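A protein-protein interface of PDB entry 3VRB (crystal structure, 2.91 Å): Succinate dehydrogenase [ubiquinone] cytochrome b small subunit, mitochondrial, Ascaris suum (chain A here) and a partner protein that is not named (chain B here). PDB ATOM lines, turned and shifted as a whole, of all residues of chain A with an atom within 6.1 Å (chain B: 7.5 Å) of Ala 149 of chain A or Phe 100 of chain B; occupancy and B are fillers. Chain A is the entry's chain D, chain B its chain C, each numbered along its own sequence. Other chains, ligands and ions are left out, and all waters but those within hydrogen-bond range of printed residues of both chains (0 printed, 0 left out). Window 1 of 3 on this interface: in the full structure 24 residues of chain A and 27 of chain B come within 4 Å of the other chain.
The backbone NH (N) of Phe 100 of chain B sits at hydrogen-bond distance from the side-chain carboxylate (OD1) of Asp 143 of chain A (3.1 Å).
The side-chain carboxylate of Asp 99 of chain B is in hydrogen-bond range of the backbone NH of Thr 101 of chain B (3.4 Å). OG1 of Thr 102 of chain B is in hydrogen-bond range of O of Asp 99 of chain B.
OD1 of Asp 143 of chain A touches CD2 of Phe 93 of chain B (3.9 Å). OD1 of Asp 143 of chain A touches CB of Asp 99 of chain B, at 3.9 Å. Phe 100 of chain B touches Val 144 of chain A (CD1 to CG2, 3.7 Å). CA of Ala 149 of chain A touches CE1 of Phe 100 of chain B (3.4 Å).
Printed residues of chain B within 4 Å of Asp 143 of chain A: Phe 93 (3.9 Å), Asp 99 (3.9 Å) and Phe 100 (3.1 Å). Printed residues of chain B within 4 Å of Val 144 of chain A: Phe 100 (3.7 Å). Printed residues of chain B within 4 Å of Ala 149 of chain A: Phe 100. Phe 150 of chain A touches none of the printed residues of chain B. Printed residues of chain A within 4 Å of Phe 93 of chain B: Asp 143 (3.9 Å). Printed residues of chain A within 4 Å of Asp 99 of chain B: Asp 143. Of chain A, only Asp 143 (3.1 Å), Val 144 (3.7 Å) and Ala 149 (3.4 Å) come within 4 Å of Phe 100 of chain B. The nearest printed residue of chain A that does not touch Phe 93 of chain B is Phe 139 of chain A (4.4 Å).
Hydrophobic or aromatic side chains of chain A within 4 Å of the printed part of chain B: Val 144 and Ala 149. Among the printed residues, 5 pairs touch across the chains. Among the printed residues, no Asp or Glu carboxylate lies within 4 Å of a Lys or Arg side-chain nitrogen of the other chain.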
ATOM      1  N   PHE A 139       5.300 -12.802 -25.827  1.00  0.00           N
ATOM      2  CA  PHE A 139       5.711 -11.436 -25.619  1.00  0.00           C
ATOM      3  C   PHE A 139       4.593 -10.528 -25.144  1.00  0.00           C
ATOM      4  O   PHE A 139       4.781  -9.734 -24.225  1.00  0.00           O
ATOM      5  CB  PHE A 139       6.324 -10.863 -26.876  1.00  0.00           C
ATOM      6  CG  PHE A 139       7.113  -9.635 -26.630  1.00  0.00           C
ATOM      7  CD1 PHE A 139       8.408  -9.724 -26.129  1.00  0.00           C
ATOM      8  CD2 PHE A 139       6.570  -8.383 -26.878  1.00  0.00           C
ATOM      9  CE1 PHE A 139       9.169  -8.573 -25.892  1.00  0.00           C
ATOM     10  CE2 PHE A 139       7.321  -7.230 -26.644  1.00  0.00           C
ATOM     11  CZ  PHE A 139       8.624  -7.329 -26.147  1.00  0.00           C
ATOM     12  N   ASP A 143       5.586  -9.811 -21.333  1.00  0.00           N
ATOM     13  CA  ASP A 143       6.428  -8.643 -21.465  1.00  0.00           C
ATOM     14  C   ASP A 143       5.563  -7.457 -21.869  1.00  0.00           C
ATOM     15  O   ASP A 143       4.333  -7.527 -21.780  1.00  0.00           O
ATOM     16  CB  ASP A 143       7.604  -8.895 -22.414  1.00  0.00           C
ATOM     17  CG  ASP A 143       8.921  -8.285 -21.897  1.00  0.00           C
ATOM     18  OD1 ASP A 143      10.006  -8.844 -22.188  1.00  0.00           O
ATOM     19  OD2 ASP A 143       8.884  -7.248 -21.192  1.00  0.00           O
ATOM     20  N   VAL A 144       6.203  -6.376 -22.299  1.00  0.00           N
ATOM     21  CA  VAL A 144       5.531  -5.092 -22.460  1.00  0.00           C
ATOM     22  C   VAL A 144       4.455  -5.074 -23.550  1.00  0.00           C
ATOM     23  O   VAL A 144       3.437  -4.395 -23.413  1.00  0.00           O
ATOM     24  CB  VAL A 144       6.527  -3.959 -22.711  1.00  0.00           C
ATOM     25  CG1 VAL A 144       6.112  -2.743 -21.913  1.00  0.00           C
ATOM     26  CG2 VAL A 144       7.918  -4.379 -22.299  1.00  0.00           C
ATOM     27  N   GLY A 145       4.666  -5.839 -24.612  1.00  0.00           N
ATOM     28  CA  GLY A 145       3.784  -5.785 -25.759  1.00  0.00           C
ATOM     29  C   GLY A 145       4.620  -5.271 -26.904  1.00  0.00           C
ATOM     30  O   GLY A 145       5.765  -4.871 -26.702  1.00  0.00           O
ATOM     31  N   LEU A 146       4.078  -5.299 -28.114  1.00  0.00           N
ATOM     32  CA  LEU A 146       4.825  -4.795 -29.243  1.00  0.00           C
ATOM     33  C   LEU A 146       4.692  -3.299 -29.339  1.00  0.00           C
ATOM     34  O   LEU A 146       5.689  -2.577 -29.305  1.00  0.00           O
ATOM     35  CB  LEU A 146       4.407  -5.480 -30.529  1.00  0.00           C
ATOM     36  CG  LEU A 146       5.534  -6.418 -30.964  1.00  0.00           C
ATOM     37  CD1 LEU A 146       5.018  -7.559 -31.842  1.00  0.00           C
ATOM     38  CD2 LEU A 146       6.647  -5.616 -31.656  1.00  0.00           C
ATOM     39  N   THR A 147       3.452  -2.833 -29.416  1.00  0.00           N
ATOM     40  CA  THR A 147       3.207  -1.411 -29.443  1.00  0.00           C
ATOM     41  C   THR A 147       4.103  -0.710 -28.416  1.00  0.00           C
ATOM     42  O   THR A 147       4.723   0.299 -28.729  1.00  0.00           O
ATOM     43  CB  THR A 147       1.704  -1.059 -29.250  1.00  0.00           C
ATOM     44  OG1 THR A 147       1.310  -1.236 -27.883  1.00  0.00           O
ATOM     45  CG2 THR A 147       0.845  -1.924 -30.130  1.00  0.00           C
ATOM     46  N   ARG A 148       4.216  -1.265 -27.210  1.00  0.00           N
ATOM     47  CA  ARG A 148       4.991  -0.603 -26.167  1.00  0.00           C
ATOM     48  C   ARG A 148       6.488  -0.729 -26.346  1.00  0.00           C
ATOM     49  O   ARG A 148       7.222   0.222 -26.088  1.00  0.00           O
ATOM     50  CB  ARG A 148       4.572  -1.049 -24.774  1.00  0.00           C
ATOM     51  CG  ARG A 148       3.651  -0.050 -24.061  1.00  0.00           C
ATOM     52  CD  ARG A 148       4.388   1.216 -23.569  1.00  0.00           C
ATOM     53  NE  ARG A 148       5.225   0.962 -22.392  1.00  0.00           N
ATOM     54  CZ  ARG A 148       6.019   1.863 -21.810  1.00  0.00           C
ATOM     55  NH1 ARG A 148       6.103   3.100 -22.283  1.00  0.00           N
ATOM     56  NH2 ARG A 148       6.732   1.521 -20.743  1.00  0.00           N
ATOM     57  N   ALA A 149       6.937  -1.892 -26.801  1.00  0.00           N
ATOM     58  CA  ALA A 149       8.353  -2.121 -27.029  1.00  0.00           C
ATOM     59  C   ALA A 149       8.915  -1.039 -27.945  1.00  0.00           C
ATOM     60  O   ALA A 149      10.022  -0.546 -27.737  1.00  0.00           O
ATOM     61  CB  ALA A 149       8.571  -3.471 -27.612  1.00  0.00           C
ATOM     62  N   PHE A 150       8.135  -0.650 -28.948  1.00  0.00           N
ATOM     63  CA  PHE A 150       8.495   0.494 -29.768  1.00  0.00           C
ATOM     64  C   PHE A 150       8.456   1.769 -28.945  1.00  0.00           C
ATOM     65  O   PHE A 150       9.461   2.463 -28.861  1.00  0.00           O
ATOM     66  CB  PHE A 150       7.617   0.614 -31.020  1.00  0.00           C
ATOM     67  CG  PHE A 150       7.959  -0.387 -32.109  1.00  0.00           C
ATOM     68  CD1 PHE A 150       7.157  -1.514 -32.320  1.00  0.00           C
ATOM     69  CD2 PHE A 150       9.079  -0.202 -32.927  1.00  0.00           C
ATOM     70  CE1 PHE A 150       7.465  -2.440 -33.327  1.00  0.00           C
ATOM     71  CE2 PHE A 150       9.394  -1.122 -33.937  1.00  0.00           C
ATOM     72  CZ  PHE A 150       8.585  -2.243 -34.136  1.00  0.00           C
ATOM     73  N   GLU A 151       7.322   2.065 -28.309  1.00  0.00           N
ATOM     74  CA  GLU A 151       7.189   3.304 -27.527  1.00  0.00           C
ATOM     75  C   GLU A 151       8.440   3.578 -26.703  1.00  0.00           C
ATOM     76  O   GLU A 151       9.000   4.676 -26.739  1.00  0.00           O
ATOM     77  CB  GLU A 151       5.979   3.251 -26.596  1.00  0.00           C
ATOM     78  CG  GLU A 151       4.632   3.210 -27.298  1.00  0.00           C
ATOM     79  CD  GLU A 151       3.470   3.572 -26.375  1.00  0.00           C
ATOM     80  OE1 GLU A 151       2.495   2.782 -26.298  1.00  0.00           O
ATOM     81  OE2 GLU A 151       3.538   4.652 -25.738  1.00  0.00           O
ATOM     82  N   MET A 152       8.881   2.554 -25.984  1.00  0.00           N
ATOM     83  CA  MET A 152      10.025   2.667 -25.103  1.00  0.00           C
ATOM     84  C   MET A 152      11.304   2.989 -25.854  1.00  0.00           C
ATOM     85  O   MET A 152      12.087   3.814 -25.394  1.00  0.00           O
ATOM     86  CB  MET A 152      10.190   1.392 -24.287  1.00  0.00           C
ATOM     87  CG  MET A 152       9.012   1.125 -23.367  1.00  0.00           C
ATOM     88  SD  MET A 152       9.205  -0.316 -22.296  1.00  0.00           S
ATOM     89  CE  MET A 152      10.376   0.294 -21.057  1.00  0.00           C
ATOM     90  N   VAL A 153      11.509   2.355 -27.009  1.00  0.00           N
ATOM     91  CA  VAL A 153      12.717   2.605 -27.804  1.00  0.00           C
ATOM     92  C   VAL A 153      12.720   3.996 -28.418  1.00  0.00           C
ATOM     93  O   VAL A 153      13.762   4.604 -28.555  1.00  0.00           O
ATOM     94  CB  VAL A 153      13.018   1.509 -28.875  1.00  0.00           C
ATOM     95  CG1 VAL A 153      13.236   0.158 -28.227  1.00  0.00           C
ATOM     96  CG2 VAL A 153      11.923   1.416 -29.893  1.00  0.00           C
ATOM     97  N   TRP A 154      11.554   4.520 -28.760  1.00  0.00           N
ATOM     98  CA  TRP A 154      11.494   5.904 -29.206  1.00  0.00           C
ATOM     99  C   TRP A 154      11.843   6.941 -28.126  1.00  0.00           C
ATOM    100  O   TRP A 154      12.422   7.980 -28.420  1.00  0.00           O
ATOM    101  CB  TRP A 154      10.157   6.211 -29.869  1.00  0.00           C
ATOM    102  CG  TRP A 154      10.291   6.396 -31.358  1.00  0.00           C
ATOM    103  CD1 TRP A 154       9.939   7.502 -32.076  1.00  0.00           C
ATOM    104  CD2 TRP A 154      10.841   5.462 -32.307  1.00  0.00           C
ATOM    105  NE1 TRP A 154      10.222   7.311 -33.410  1.00  0.00           N
ATOM    106  CE2 TRP A 154      10.774   6.069 -33.577  1.00  0.00           C
ATOM    107  CE3 TRP A 154      11.362   4.173 -32.208  1.00  0.00           C
ATOM    108  CZ2 TRP A 154      11.209   5.432 -34.732  1.00  0.00           C
ATOM    109  CZ3 TRP A 154      11.795   3.540 -33.361  1.00  0.00           C
ATOM    110  CH2 TRP A 154      11.712   4.169 -34.605  1.00  0.00           C
ATOM    111  N   PHE B  93      13.626 -13.349 -25.473  1.00  0.00           N
ATOM    112  CA  PHE B  93      13.102 -12.870 -24.193  1.00  0.00           C
ATOM    113  C   PHE B  93      12.323 -13.897 -23.362  1.00  0.00           C
ATOM    114  O   PHE B  93      12.084 -13.681 -22.161  1.00  0.00           O
ATOM    115  CB  PHE B  93      12.268 -11.605 -24.414  1.00  0.00           C
ATOM    116  CG  PHE B  93      13.072 -10.442 -24.897  1.00  0.00           C
ATOM    117  CD1 PHE B  93      13.501 -10.375 -26.224  1.00  0.00           C
ATOM    118  CD2 PHE B  93      13.423  -9.424 -24.027  1.00  0.00           C
ATOM    119  CE1 PHE B  93      14.262  -9.304 -26.684  1.00  0.00           C
ATOM    120  CE2 PHE B  93      14.183  -8.349 -24.466  1.00  0.00           C
ATOM    121  CZ  PHE B  93      14.599  -8.283 -25.798  1.00  0.00           C
ATOM    122  N   LEU B  98      16.009 -12.336 -18.980  1.00  0.00           N
ATOM    123  CA  LEU B  98      16.449 -10.951 -19.123  1.00  0.00           C
ATOM    124  C   LEU B  98      15.402 -10.160 -19.894  1.00  0.00           C
ATOM    125  O   LEU B  98      15.563  -9.911 -21.084  1.00  0.00           O
ATOM    126  CB  LEU B  98      17.821 -10.878 -19.828  1.00  0.00           C
ATOM    127  CG  LEU B  98      19.067 -11.604 -19.271  1.00  0.00           C
ATOM    128  CD1 LEU B  98      19.182 -13.029 -19.800  1.00  0.00           C
ATOM    129  CD2 LEU B  98      20.373 -10.849 -19.576  1.00  0.00           C
ATOM    130  N   ASP B  99      14.336  -9.759 -19.205  1.00  0.00           N
ATOM    131  CA  ASP B  99      13.174  -9.155 -19.855  1.00  0.00           C
ATOM    132  C   ASP B  99      13.488  -7.830 -20.543  1.00  0.00           C
ATOM    133  O   ASP B  99      14.612  -7.335 -20.466  1.00  0.00           O
ATOM    134  CB  ASP B  99      12.021  -8.996 -18.859  1.00  0.00           C
ATOM    135  CG  ASP B  99      12.052  -7.673 -18.107  1.00  0.00           C
ATOM    136  OD1 ASP B  99      13.088  -6.975 -18.134  1.00  0.00           O
ATOM    137  OD2 ASP B  99      11.022  -7.329 -17.484  1.00  0.00           O
ATOM    138  N   PHE B 100      12.479  -7.249 -21.189  1.00  0.00           N
ATOM    139  CA  PHE B 100      12.670  -6.090 -22.046  1.00  0.00           C
ATOM    140  C   PHE B 100      13.045  -4.845 -21.295  1.00  0.00           C
ATOM    141  O   PHE B 100      14.063  -4.234 -21.591  1.00  0.00           O
ATOM    142  CB  PHE B 100      11.414  -5.814 -22.831  1.00  0.00           C
ATOM    143  CG  PHE B 100      11.644  -5.010 -24.054  1.00  0.00           C
ATOM    144  CD1 PHE B 100      10.993  -3.801 -24.235  1.00  0.00           C
ATOM    145  CD2 PHE B 100      12.499  -5.463 -25.048  1.00  0.00           C
ATOM    146  CE1 PHE B 100      11.196  -3.049 -25.394  1.00  0.00           C
ATOM    147  CE2 PHE B 100      12.707  -4.721 -26.206  1.00  0.00           C
ATOM    148  CZ  PHE B 100      12.053  -3.511 -26.377  1.00  0.00           C
ATOM    149  N   THR B 101      12.218  -4.479 -20.320  1.00  0.00           N
ATOM    150  CA  THR B 101      12.423  -3.273 -19.514  1.00  0.00           C
ATOM    151  C   THR B 101      13.879  -3.092 -19.091  1.00  0.00           C
ATOM    152  O   THR B 101      14.472  -2.028 -19.307  1.00  0.00           O
ATOM    153  CB  THR B 101      11.534  -3.283 -18.261  1.00  0.00           C
ATOM    154  OG1 THR B 101      10.220  -3.716 -18.621  1.00  0.00           O
ATOM    155  CG2 THR B 101      11.453  -1.888 -17.632  1.00  0.00           C
ATOM    156  N   THR B 102      14.446  -4.138 -18.496  1.00  0.00           N
ATOM    157  CA  THR B 102      15.827  -4.112 -18.024  1.00  0.00           C
ATOM    158  C   THR B 102      16.813  -3.924 -19.180  1.00  0.00           C
ATOM    159  O   THR B 102      17.791  -3.194 -19.054  1.00  0.00           O
ATOM    160  CB  THR B 102      16.169  -5.386 -17.252  1.00  0.00           C
ATOM    161  OG1 THR B 102      16.060  -6.512 -18.127  1.00  0.00           O
ATOM    162  CG2 THR B 102      15.209  -5.573 -16.084  1.00  0.00           C
ATOM    163  N   PHE B 103      16.544  -4.572 -20.306  1.00  0.00           N
ATOM    164  CA  PHE B 103      17.382  -4.407 -21.473  1.00  0.00           C
ATOM    165  C   PHE B 103      17.341  -2.957 -21.924  1.00  0.00           C
ATOM    166  O   PHE B 103      18.385  -2.330 -22.137  1.00  0.00           O
ATOM    167  CB  PHE B 103      16.931  -5.330 -22.594  1.00  0.00           C
ATOM    168  CG  PHE B 103      17.478  -4.960 -23.950  1.00  0.00           C
ATOM    169  CD1 PHE B 103      18.805  -5.237 -24.287  1.00  0.00           C
ATOM    170  CD2 PHE B 103      16.658  -4.345 -24.908  1.00  0.00           C
ATOM    171  CE1 PHE B 103      19.314  -4.904 -25.556  1.00  0.00           C
ATOM    172  CE2 PHE B 103      17.153  -4.007 -26.182  1.00  0.00           C
ATOM    173  CZ  PHE B 103      18.485  -4.287 -26.505  1.00  0.00           C
ATOM    174  N   VAL B 104      16.131  -2.420 -22.042  1.00  0.00           N
ATOM    175  CA  VAL B 104      15.926  -1.064 -22.543  1.00  0.00           C
ATOM    176  C   VAL B 104      16.825  -0.050 -21.853  1.00  0.00           C
ATOM    177  O   VAL B 104      17.099   1.002 -22.411  1.00  0.00           O
ATOM    178  CB  VAL B 104      14.467  -0.590 -22.384  1.00  0.00           C
ATOM    179  CG1 VAL B 104      14.188   0.596 -23.290  1.00  0.00           C
ATOM    180  CG2 VAL B 104      13.497  -1.700 -22.694  1.00  0.00           C
ATOM    181  N   GLU B 105      17.288  -0.348 -20.644  1.00  0.00           N
ATOM    182  CA  GLU B 105      18.116   0.631 -19.942  1.00  0.00           C
ATOM    183  C   GLU B 105      19.543   0.207 -19.572  1.00  0.00           C
ATOM    184  O   GLU B 105      20.403   1.067 -19.319  1.00  0.00           O
ATOM    185  CB  GLU B 105      17.362   1.279 -18.774  1.00  0.00           C
ATOM    186  CG  GLU B 105      16.516   0.334 -17.966  1.00  0.00           C
ATOM    187  CD  GLU B 105      16.595   0.658 -16.495  1.00  0.00           C
ATOM    188  OE1 GLU B 105      17.242  -0.126 -15.763  1.00  0.00           O
ATOM    189  OE2 GLU B 105      16.046   1.706 -16.078  1.00  0.00           O
ATOM    190  N   PHE B 106      19.802  -1.104 -19.562  1.00  0.00           N
ATOM    191  CA  PHE B 106      21.184  -1.616 -19.616  1.00  0.00           C
ATOM    192  C   PHE B 106      21.705  -1.275 -21.019  1.00  0.00           C
ATOM    193  O   PHE B 106      22.699  -1.841 -21.491  1.00  0.00           O
ATOM    194  CB  PHE B 106      21.263  -3.133 -19.317  1.00  0.00           C
ATOM    195  CG  PHE B 106      21.429  -3.492 -17.824  1.00  0.00           C
ATOM    196  CD1 PHE B 106      20.653  -2.863 -16.818  1.00  0.00           C
ATOM    197  CD2 PHE B 106      22.332  -4.500 -17.434  1.00  0.00           C
ATOM    198  CE1 PHE B 106      20.800  -3.211 -15.448  1.00  0.00           C
ATOM    199  CE2 PHE B 106      22.484  -4.859 -16.070  1.00  0.00           C
ATOM    200  CZ  PHE B 106      21.714  -4.214 -15.077  1.00  0.00           C
